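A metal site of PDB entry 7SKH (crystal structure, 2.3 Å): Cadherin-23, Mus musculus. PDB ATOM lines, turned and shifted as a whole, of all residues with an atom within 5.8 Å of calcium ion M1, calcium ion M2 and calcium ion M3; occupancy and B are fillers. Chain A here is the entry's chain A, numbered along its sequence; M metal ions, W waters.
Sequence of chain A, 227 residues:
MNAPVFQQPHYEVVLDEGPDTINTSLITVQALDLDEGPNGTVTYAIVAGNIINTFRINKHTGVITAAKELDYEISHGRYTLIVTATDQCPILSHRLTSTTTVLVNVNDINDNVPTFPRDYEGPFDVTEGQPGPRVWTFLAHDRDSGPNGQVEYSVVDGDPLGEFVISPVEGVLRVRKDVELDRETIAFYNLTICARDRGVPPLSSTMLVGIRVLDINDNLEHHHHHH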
ATOM      1  N   GLU A  17     -28.355 -23.394  -3.720  1.00  0.00           N
ATOM      2  CA  GLU A  17     -28.217 -22.451  -2.600  1.00  0.00           C
ATOM      3  C   GLU A  17     -27.116 -21.445  -2.960  1.00  0.00           C
ATOM      4  O   GLU A  17     -26.393 -21.685  -3.929  1.00  0.00           O
ATOM      5  CB  GLU A  17     -27.856 -23.188  -1.317  1.00  0.00           C
ATOM      6  CG  GLU A  17     -26.417 -23.664  -1.293  1.00  0.00           C
ATOM      7  CD  GLU A  17     -25.990 -24.153   0.073  1.00  0.00           C
ATOM      8  OE1 GLU A  17     -25.161 -25.115   0.133  1.00  0.00           O
ATOM      9  OE2 GLU A  17     -26.473 -23.563   1.090  1.00  0.00           O
ATOM     10  N   GLU A  69     -30.732 -15.343   1.561  1.00  0.00           N
ATOM     11  CA  GLU A  69     -29.984 -16.380   0.836  1.00  0.00           C
ATOM     12  C   GLU A  69     -30.663 -17.746   1.046  1.00  0.00           C
ATOM     13  O   GLU A  69     -30.965 -18.122   2.180  1.00  0.00           O
ATOM     14  CB  GLU A  69     -28.552 -16.309   1.351  1.00  0.00           C
ATOM     15  CG  GLU A  69     -27.627 -17.182   0.577  1.00  0.00           C
ATOM     16  CD  GLU A  69     -26.242 -17.201   1.161  1.00  0.00           C
ATOM     17  OE1 GLU A  69     -25.892 -16.197   1.781  1.00  0.00           O
ATOM     18  OE2 GLU A  69     -25.544 -18.231   0.995  1.00  0.00           O
ATOM     19  N   LEU A  70     -30.938 -18.459  -0.034  1.00  0.00           N
ATOM     20  CA  LEU A  70     -31.344 -19.879   0.036  1.00  0.00           C
ATOM     21  C   LEU A  70     -30.158 -20.641   0.572  1.00  0.00           C
ATOM     22  O   LEU A  70     -29.038 -20.392   0.115  1.00  0.00           O
ATOM     23  CB  LEU A  70     -31.722 -20.348  -1.359  1.00  0.00           C
ATOM     24  CG  LEU A  70     -32.982 -19.709  -1.941  1.00  0.00           C
ATOM     25  CD1 LEU A  70     -33.529 -20.558  -3.073  1.00  0.00           C
ATOM     26  CD2 LEU A  70     -34.040 -19.537  -0.861  1.00  0.00           C
ATOM     27  N   ASP A  71     -30.393 -21.514   1.512  1.00  0.00           N
ATOM     28  CA  ASP A  71     -29.333 -22.149   2.324  1.00  0.00           C
ATOM     29  C   ASP A  71     -29.729 -23.609   2.485  1.00  0.00           C
ATOM     30  O   ASP A  71     -30.763 -23.889   3.128  1.00  0.00           O
ATOM     31  CB  ASP A  71     -29.177 -21.475   3.686  1.00  0.00           C
ATOM     32  CG  ASP A  71     -28.060 -22.064   4.537  1.00  0.00           C
ATOM     33  OD1 ASP A  71     -27.186 -22.774   3.955  1.00  0.00           O
ATOM     34  OD2 ASP A  71     -28.067 -21.842   5.755  1.00  0.00           O
ATOM     35  N   TYR A  72     -28.926 -24.500   1.909  1.00  0.00           N
ATOM     36  CA  TYR A  72     -29.114 -25.955   2.074  1.00  0.00           C
ATOM     37  C   TYR A  72     -29.009 -26.314   3.552  1.00  0.00           C
ATOM     38  O   TYR A  72     -29.689 -27.239   3.956  1.00  0.00           O
ATOM     39  CB  TYR A  72     -28.094 -26.729   1.243  1.00  0.00           C
ATOM     40  CG  TYR A  72     -28.383 -28.207   1.187  1.00  0.00           C
ATOM     41  CD1 TYR A  72     -27.929 -29.039   2.184  1.00  0.00           C
ATOM     42  CD2 TYR A  72     -29.106 -28.763   0.142  1.00  0.00           C
ATOM     43  CE1 TYR A  72     -28.162 -30.404   2.136  1.00  0.00           C
ATOM     44  CE2 TYR A  72     -29.379 -30.120   0.092  1.00  0.00           C
ATOM     45  CZ  TYR A  72     -28.891 -30.943   1.084  1.00  0.00           C
ATOM     46  OH  TYR A  72     -29.116 -32.293   1.092  1.00  0.00           O
ATOM     47  N   GLU A  73     -28.152 -25.634   4.318  1.00  0.00           N
ATOM     48  CA  GLU A  73     -27.854 -26.057   5.700  1.00  0.00           C
ATOM     49  C   GLU A  73     -29.037 -25.724   6.611  1.00  0.00           C
ATOM     50  O   GLU A  73     -29.174 -26.376   7.627  1.00  0.00           O
ATOM     51  CB  GLU A  73     -26.538 -25.448   6.189  1.00  0.00           C
ATOM     52  CG  GLU A  73     -25.301 -26.128   5.629  1.00  0.00           C
ATOM     53  CD  GLU A  73     -25.054 -26.036   4.121  1.00  0.00           C
ATOM     54  OE1 GLU A  73     -24.981 -24.950   3.588  1.00  0.00           O
ATOM     55  OE2 GLU A  73     -24.859 -27.069   3.476  1.00  0.00           O
ATOM     56  N   ASP A 108     -27.080 -28.561  -2.519  1.00  0.00           N
ATOM     57  CA  ASP A 108     -25.927 -28.285  -1.630  1.00  0.00           C
ATOM     58  C   ASP A 108     -24.730 -27.802  -2.466  1.00  0.00           C
ATOM     59  O   ASP A 108     -24.438 -28.431  -3.449  1.00  0.00           O
ATOM     60  CB  ASP A 108     -25.574 -29.524  -0.826  1.00  0.00           C
ATOM     61  CG  ASP A 108     -24.538 -29.306   0.268  1.00  0.00           C
ATOM     62  OD1 ASP A 108     -24.447 -28.174   0.807  1.00  0.00           O
ATOM     63  OD2 ASP A 108     -23.850 -30.286   0.598  1.00  0.00           O
ATOM     64  N   ILE A 109     -24.115 -26.667  -2.105  1.00  0.00           N
ATOM     65  CA  ILE A 109     -22.759 -26.271  -2.619  1.00  0.00           C
ATOM     66  C   ILE A 109     -21.768 -26.317  -1.441  1.00  0.00           C
ATOM     67  O   ILE A 109     -22.191 -26.229  -0.262  1.00  0.00           O
ATOM     68  CB  ILE A 109     -22.776 -24.889  -3.325  1.00  0.00           C
ATOM     69  CG1 ILE A 109     -22.828 -23.710  -2.357  1.00  0.00           C
ATOM     70  CG2 ILE A 109     -23.904 -24.818  -4.353  1.00  0.00           C
ATOM     71  CD1 ILE A 109     -22.795 -22.323  -3.033  1.00  0.00           C
ATOM     72  N   ASN A 110     -20.490 -26.403  -1.769  1.00  0.00           N
ATOM     73  CA  ASN A 110     -19.403 -26.480  -0.776  1.00  0.00           C
ATOM     74  C   ASN A 110     -19.154 -25.055  -0.260  1.00  0.00           C
ATOM     75  O   ASN A 110     -18.223 -24.395  -0.772  1.00  0.00           O
ATOM     76  CB  ASN A 110     -18.166 -27.157  -1.353  1.00  0.00           C
ATOM     77  CG  ASN A 110     -17.234 -27.594  -0.253  1.00  0.00           C
ATOM     78  OD1 ASN A 110     -17.685 -27.946   0.840  1.00  0.00           O
ATOM     79  ND2 ASN A 110     -15.942 -27.639  -0.548  1.00  0.00           N
ATOM     80  N   ASP A 111     -19.967 -24.602   0.695  1.00  0.00           N
ATOM     81  CA  ASP A 111     -19.846 -23.250   1.306  1.00  0.00           C
ATOM     82  C   ASP A 111     -19.518 -23.354   2.809  1.00  0.00           C
ATOM     83  O   ASP A 111     -19.611 -22.313   3.469  1.00  0.00           O
ATOM     84  CB  ASP A 111     -21.096 -22.388   1.042  1.00  0.00           C
ATOM     85  CG  ASP A 111     -22.428 -22.972   1.520  1.00  0.00           C
ATOM     86  OD1 ASP A 111     -22.477 -24.185   1.859  1.00  0.00           O
ATOM     87  OD2 ASP A 111     -23.406 -22.212   1.558  1.00  0.00           O
ATOM     88  N   ASN A 112     -19.169 -24.529   3.354  1.00  0.00           N
ATOM     89  CA  ASN A 112     -18.744 -24.681   4.769  1.00  0.00           C
ATOM     90  C   ASN A 112     -17.345 -25.320   4.791  1.00  0.00           C
ATOM     91  O   ASN A 112     -17.133 -26.354   4.103  1.00  0.00           O
ATOM     92  CB  ASN A 112     -19.791 -25.416   5.614  1.00  0.00           C
ATOM     93  CG  ASN A 112     -21.061 -24.589   5.753  1.00  0.00           C
ATOM     94  OD1 ASN A 112     -21.152 -23.752   6.636  1.00  0.00           O
ATOM     95  ND2 ASN A 112     -22.008 -24.767   4.850  1.00  0.00           N
ATOM     96  N   VAL A 113     -16.423 -24.666   5.493  1.00  0.00           N
ATOM     97  CA  VAL A 113     -15.020 -25.110   5.713  1.00  0.00           C
ATOM     98  C   VAL A 113     -15.043 -26.179   6.803  1.00  0.00           C
ATOM     99  O   VAL A 113     -15.745 -26.001   7.797  1.00  0.00           O
ATOM    100  CB  VAL A 113     -14.151 -23.915   6.149  1.00  0.00           C
ATOM    101  CG1 VAL A 113     -12.695 -24.305   6.261  1.00  0.00           C
ATOM    102  CG2 VAL A 113     -14.299 -22.709   5.233  1.00  0.00           C
ATOM    103  N   PRO A 114     -14.316 -27.312   6.639  1.00  0.00           N
ATOM    104  CA  PRO A 114     -14.196 -28.293   7.715  1.00  0.00           C
ATOM    105  C   PRO A 114     -13.445 -27.592   8.843  1.00  0.00           C
ATOM    106  O   PRO A 114     -12.365 -27.131   8.578  1.00  0.00           O
ATOM    107  CB  PRO A 114     -13.383 -29.443   7.132  1.00  0.00           C
ATOM    108  CG  PRO A 114     -12.773 -28.902   5.842  1.00  0.00           C
ATOM    109  CD  PRO A 114     -13.580 -27.702   5.429  1.00  0.00           C
ATOM    110  N   ASP A 142     -17.895 -30.501   9.365  1.00  0.00           N
ATOM    111  CA  ASP A 142     -18.263 -29.831   8.090  1.00  0.00           C
ATOM    112  C   ASP A 142     -19.790 -29.813   7.983  1.00  0.00           C
ATOM    113  O   ASP A 142     -20.378 -30.869   7.880  1.00  0.00           O
ATOM    114  CB  ASP A 142     -17.557 -30.521   6.919  1.00  0.00           C
ATOM    115  CG  ASP A 142     -17.569 -29.675   5.673  1.00  0.00           C
ATOM    116  OD1 ASP A 142     -18.668 -29.218   5.289  1.00  0.00           O
ATOM    117  OD2 ASP A 142     -16.493 -29.477   5.097  1.00  0.00           O
ATOM    118  N   ARG A 143     -20.387 -28.636   7.926  1.00  0.00           N
ATOM    119  CA  ARG A 143     -21.863 -28.441   7.962  1.00  0.00           C
ATOM    120  C   ARG A 143     -22.493 -28.887   6.638  1.00  0.00           C
ATOM    121  O   ARG A 143     -23.702 -29.054   6.619  1.00  0.00           O
ATOM    122  CB  ARG A 143     -22.199 -26.968   8.248  1.00  0.00           C
ATOM    123  CG  ARG A 143     -22.090 -26.580   9.724  1.00  0.00           C
ATOM    124  CD  ARG A 143     -22.179 -25.071   9.949  1.00  0.00           C
ATOM    125  NE  ARG A 143     -23.563 -24.584   9.960  1.00  0.00           N
ATOM    126  CZ  ARG A 143     -24.150 -23.928   8.971  1.00  0.00           C
ATOM    127  NH1 ARG A 143     -23.495 -23.621   7.876  1.00  0.00           N
ATOM    128  NH2 ARG A 143     -25.404 -23.567   9.094  1.00  0.00           N
ATOM    129  N   ASP A 144     -21.703 -29.024   5.561  1.00  0.00           N
ATOM    130  CA  ASP A 144     -22.235 -29.490   4.245  1.00  0.00           C
ATOM    131  C   ASP A 144     -22.598 -30.968   4.305  1.00  0.00           C
ATOM    132  O   ASP A 144     -22.329 -31.621   5.314  1.00  0.00           O
ATOM    133  CB  ASP A 144     -21.245 -29.231   3.087  1.00  0.00           C
ATOM    134  CG  ASP A 144     -20.834 -27.775   2.959  1.00  0.00           C
ATOM    135  OD1 ASP A 144     -21.719 -26.930   2.908  1.00  0.00           O
ATOM    136  OD2 ASP A 144     -19.630 -27.505   2.957  1.00  0.00           O
ATOM    137  N   SER A 145     -23.250 -31.447   3.253  1.00  0.00           N
ATOM    138  CA  SER A 145     -23.699 -32.840   3.064  1.00  0.00           C
ATOM    139  C   SER A 145     -22.971 -33.486   1.873  1.00  0.00           C
ATOM    140  O   SER A 145     -22.256 -32.783   1.143  1.00  0.00           O
ATOM    141  CB  SER A 145     -25.196 -32.877   2.882  1.00  0.00           C
ATOM    142  OG  SER A 145     -25.799 -32.457   4.082  1.00  0.00           O
ATOM    143  N   ASN A 148     -19.215 -32.873  -0.075  1.00  0.00           N
ATOM    144  CA  ASN A 148     -19.002 -31.485   0.379  1.00  0.00           C
ATOM    145  C   ASN A 148     -18.784 -31.511   1.889  1.00  0.00           C
ATOM    146  O   ASN A 148     -18.126 -30.641   2.396  1.00  0.00           O
ATOM    147  CB  ASN A 148     -20.183 -30.592   0.025  1.00  0.00           C
ATOM    148  CG  ASN A 148     -20.339 -30.261  -1.452  1.00  0.00           C
ATOM    149  OD1 ASN A 148     -19.389 -30.274  -2.218  1.00  0.00           O
ATOM    150  ND2 ASN A 148     -21.546 -29.864  -1.811  1.00  0.00           N
ATOM    151  N   GLY A 149     -19.373 -32.479   2.582  1.00  0.00           N
ATOM    152  CA  GLY A 149     -19.286 -32.615   4.040  1.00  0.00           C
ATOM    153  C   GLY A 149     -18.324 -33.668   4.519  1.00  0.00           C
ATOM    154  O   GLY A 149     -18.240 -33.829   5.750  1.00  0.00           O
ATOM    155  N   ASP A 197     -12.156 -31.152   2.856  1.00  0.00           N
ATOM    156  CA  ASP A 197     -13.430 -31.804   2.449  1.00  0.00           C
ATOM    157  C   ASP A 197     -13.275 -32.330   1.028  1.00  0.00           C
ATOM    158  O   ASP A 197     -12.233 -32.120   0.427  1.00  0.00           O
ATOM    159  CB  ASP A 197     -14.618 -30.885   2.692  1.00  0.00           C
ATOM    160  CG  ASP A 197     -14.639 -29.662   1.822  1.00  0.00           C
ATOM    161  OD1 ASP A 197     -14.049 -29.719   0.720  1.00  0.00           O
ATOM    162  OD2 ASP A 197     -15.276 -28.686   2.222  1.00  0.00           O
ATOM    163  N   LEU A 203     -12.451 -27.227   0.404  1.00  0.00           N
ATOM    164  CA  LEU A 203     -12.138 -26.262   1.486  1.00  0.00           C
ATOM    165  C   LEU A 203     -11.385 -27.039   2.568  1.00  0.00           C
ATOM    166  O   LEU A 203     -11.694 -28.263   2.761  1.00  0.00           O
ATOM    167  CB  LEU A 203     -13.414 -25.619   2.015  1.00  0.00           C
ATOM    168  CG  LEU A 203     -14.234 -24.771   1.025  1.00  0.00           C
ATOM    169  CD1 LEU A 203     -15.604 -24.460   1.593  1.00  0.00           C
ATOM    170  CD2 LEU A 203     -13.509 -23.487   0.632  1.00  0.00           C
HETATM  171 CA    CA M   1     -17.495 -28.436   3.122  1.00  0.00          CA
HETATM  172 CA    CA M   2     -23.681 -26.171   1.619  1.00  0.00          CA
HETATM  173 CA    CA M   3     -25.218 -22.844   2.873  1.00  0.00          CA
HETATM  174  O   HOH W   1     -26.020 -20.440   2.497  1.00  0.00           O
HETATM  175  O   HOH W   2     -23.935 -22.399   4.848  1.00  0.00           O
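O of Asn 112 binds calcium ion M1, 2.3 Å away.
Calcium ion M1 is bound by the side-chain carboxylate (OD2) of Asp 144 (2.3 Å).
Calcium ion M1 is bound by the side-chain amide oxygen (OD1) of Asn 110 (2.3 Å).
Calcium ion M1 is bound by O of Asn 148, at 2.4 Å.
OD2 of Asp 197 is bound to calcium ion M1 (2.4 Å).
OD2 of Asp 142 is bound to calcium ion M1 (2.4 Å).
OD1 of Asp 142 is bound to calcium ion M1, 2.6 Å away.
Calcium ion M1 has seven donor atoms within binding distance.
Of the 21 residues printed, 7 come within 4 Å of calcium ion M2.
Of the 21 residues printed, 4 come within 4 Å of calcium ion M3.
The nearest printed residue that does not touch calcium ion M3 is Tyr 72 (4.2 Å).
Calcium ion M2 is bound by OD1 of Asp 108 (2.3 Å), OD1 of Asp 111 (2.3 Å), OE1 of Glu 17 (2.3 Å), OE2 of Glu 73 (2.4 Å), O of Ile 109 (2.4 Å), OD1 of Asp 144 (2.5 Å) and OE1 of Glu 73 (2.7 Å).
Calcium ion M2 has seven donor atoms within binding distance.
Six residues have an atom within 4 Å of calcium ion M1: Asn 110, Asn 112, Asp 142, Asp 144, Asn 148 and Asp 197.
OE1 of Glu 73 is bound to calcium ion M3 (2.2 Å).
The side-chain carboxylate (OD1) of Asp 71 binds calcium ion M3 (2.2 Å).
OE2 of Glu 17 is bound to calcium ion M3 (2.3 Å).
Calcium ion M3 is bound by the side-chain carboxylate (OD2) of Asp 111.
Calcium ion M3 is bound by water W2, 2.4 Å away.
Water W1 binds calcium ion M3, at 2.6 Å.
OE1 of Glu 73 lies close to ND2 of Asn 112.
The side-chain amide nitrogen (ND2) of Asn 148 lies within hydrogen-bond range of the side-chain carboxylate (OD2) of Asp 108, at 3.4 Å.
The backbone NH of Ser 145 sits at hydrogen-bond distance from the side-chain carboxylate of Asp 108, at 3.0 Å.
N of Tyr 72 lies close to OE2 of Glu 17 (2.8 Å).
OD1 of Asp 111 lies close to ND2 of Asn 112.
The guanidinium group of Arg 143 sits at hydrogen-bond distance from the side-chain amide oxygen of Asn 112 (2.7 Å).
The backbone carbonyl oxygen (O) of Leu 203 sits at hydrogen-bond distance from the backbone NH (N) of Asp 197, 2.9 Å away.
Water W2 bridges ND2 of Asn 112 (3.1 Å) and NH1 of Arg 143 (3.3 Å).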
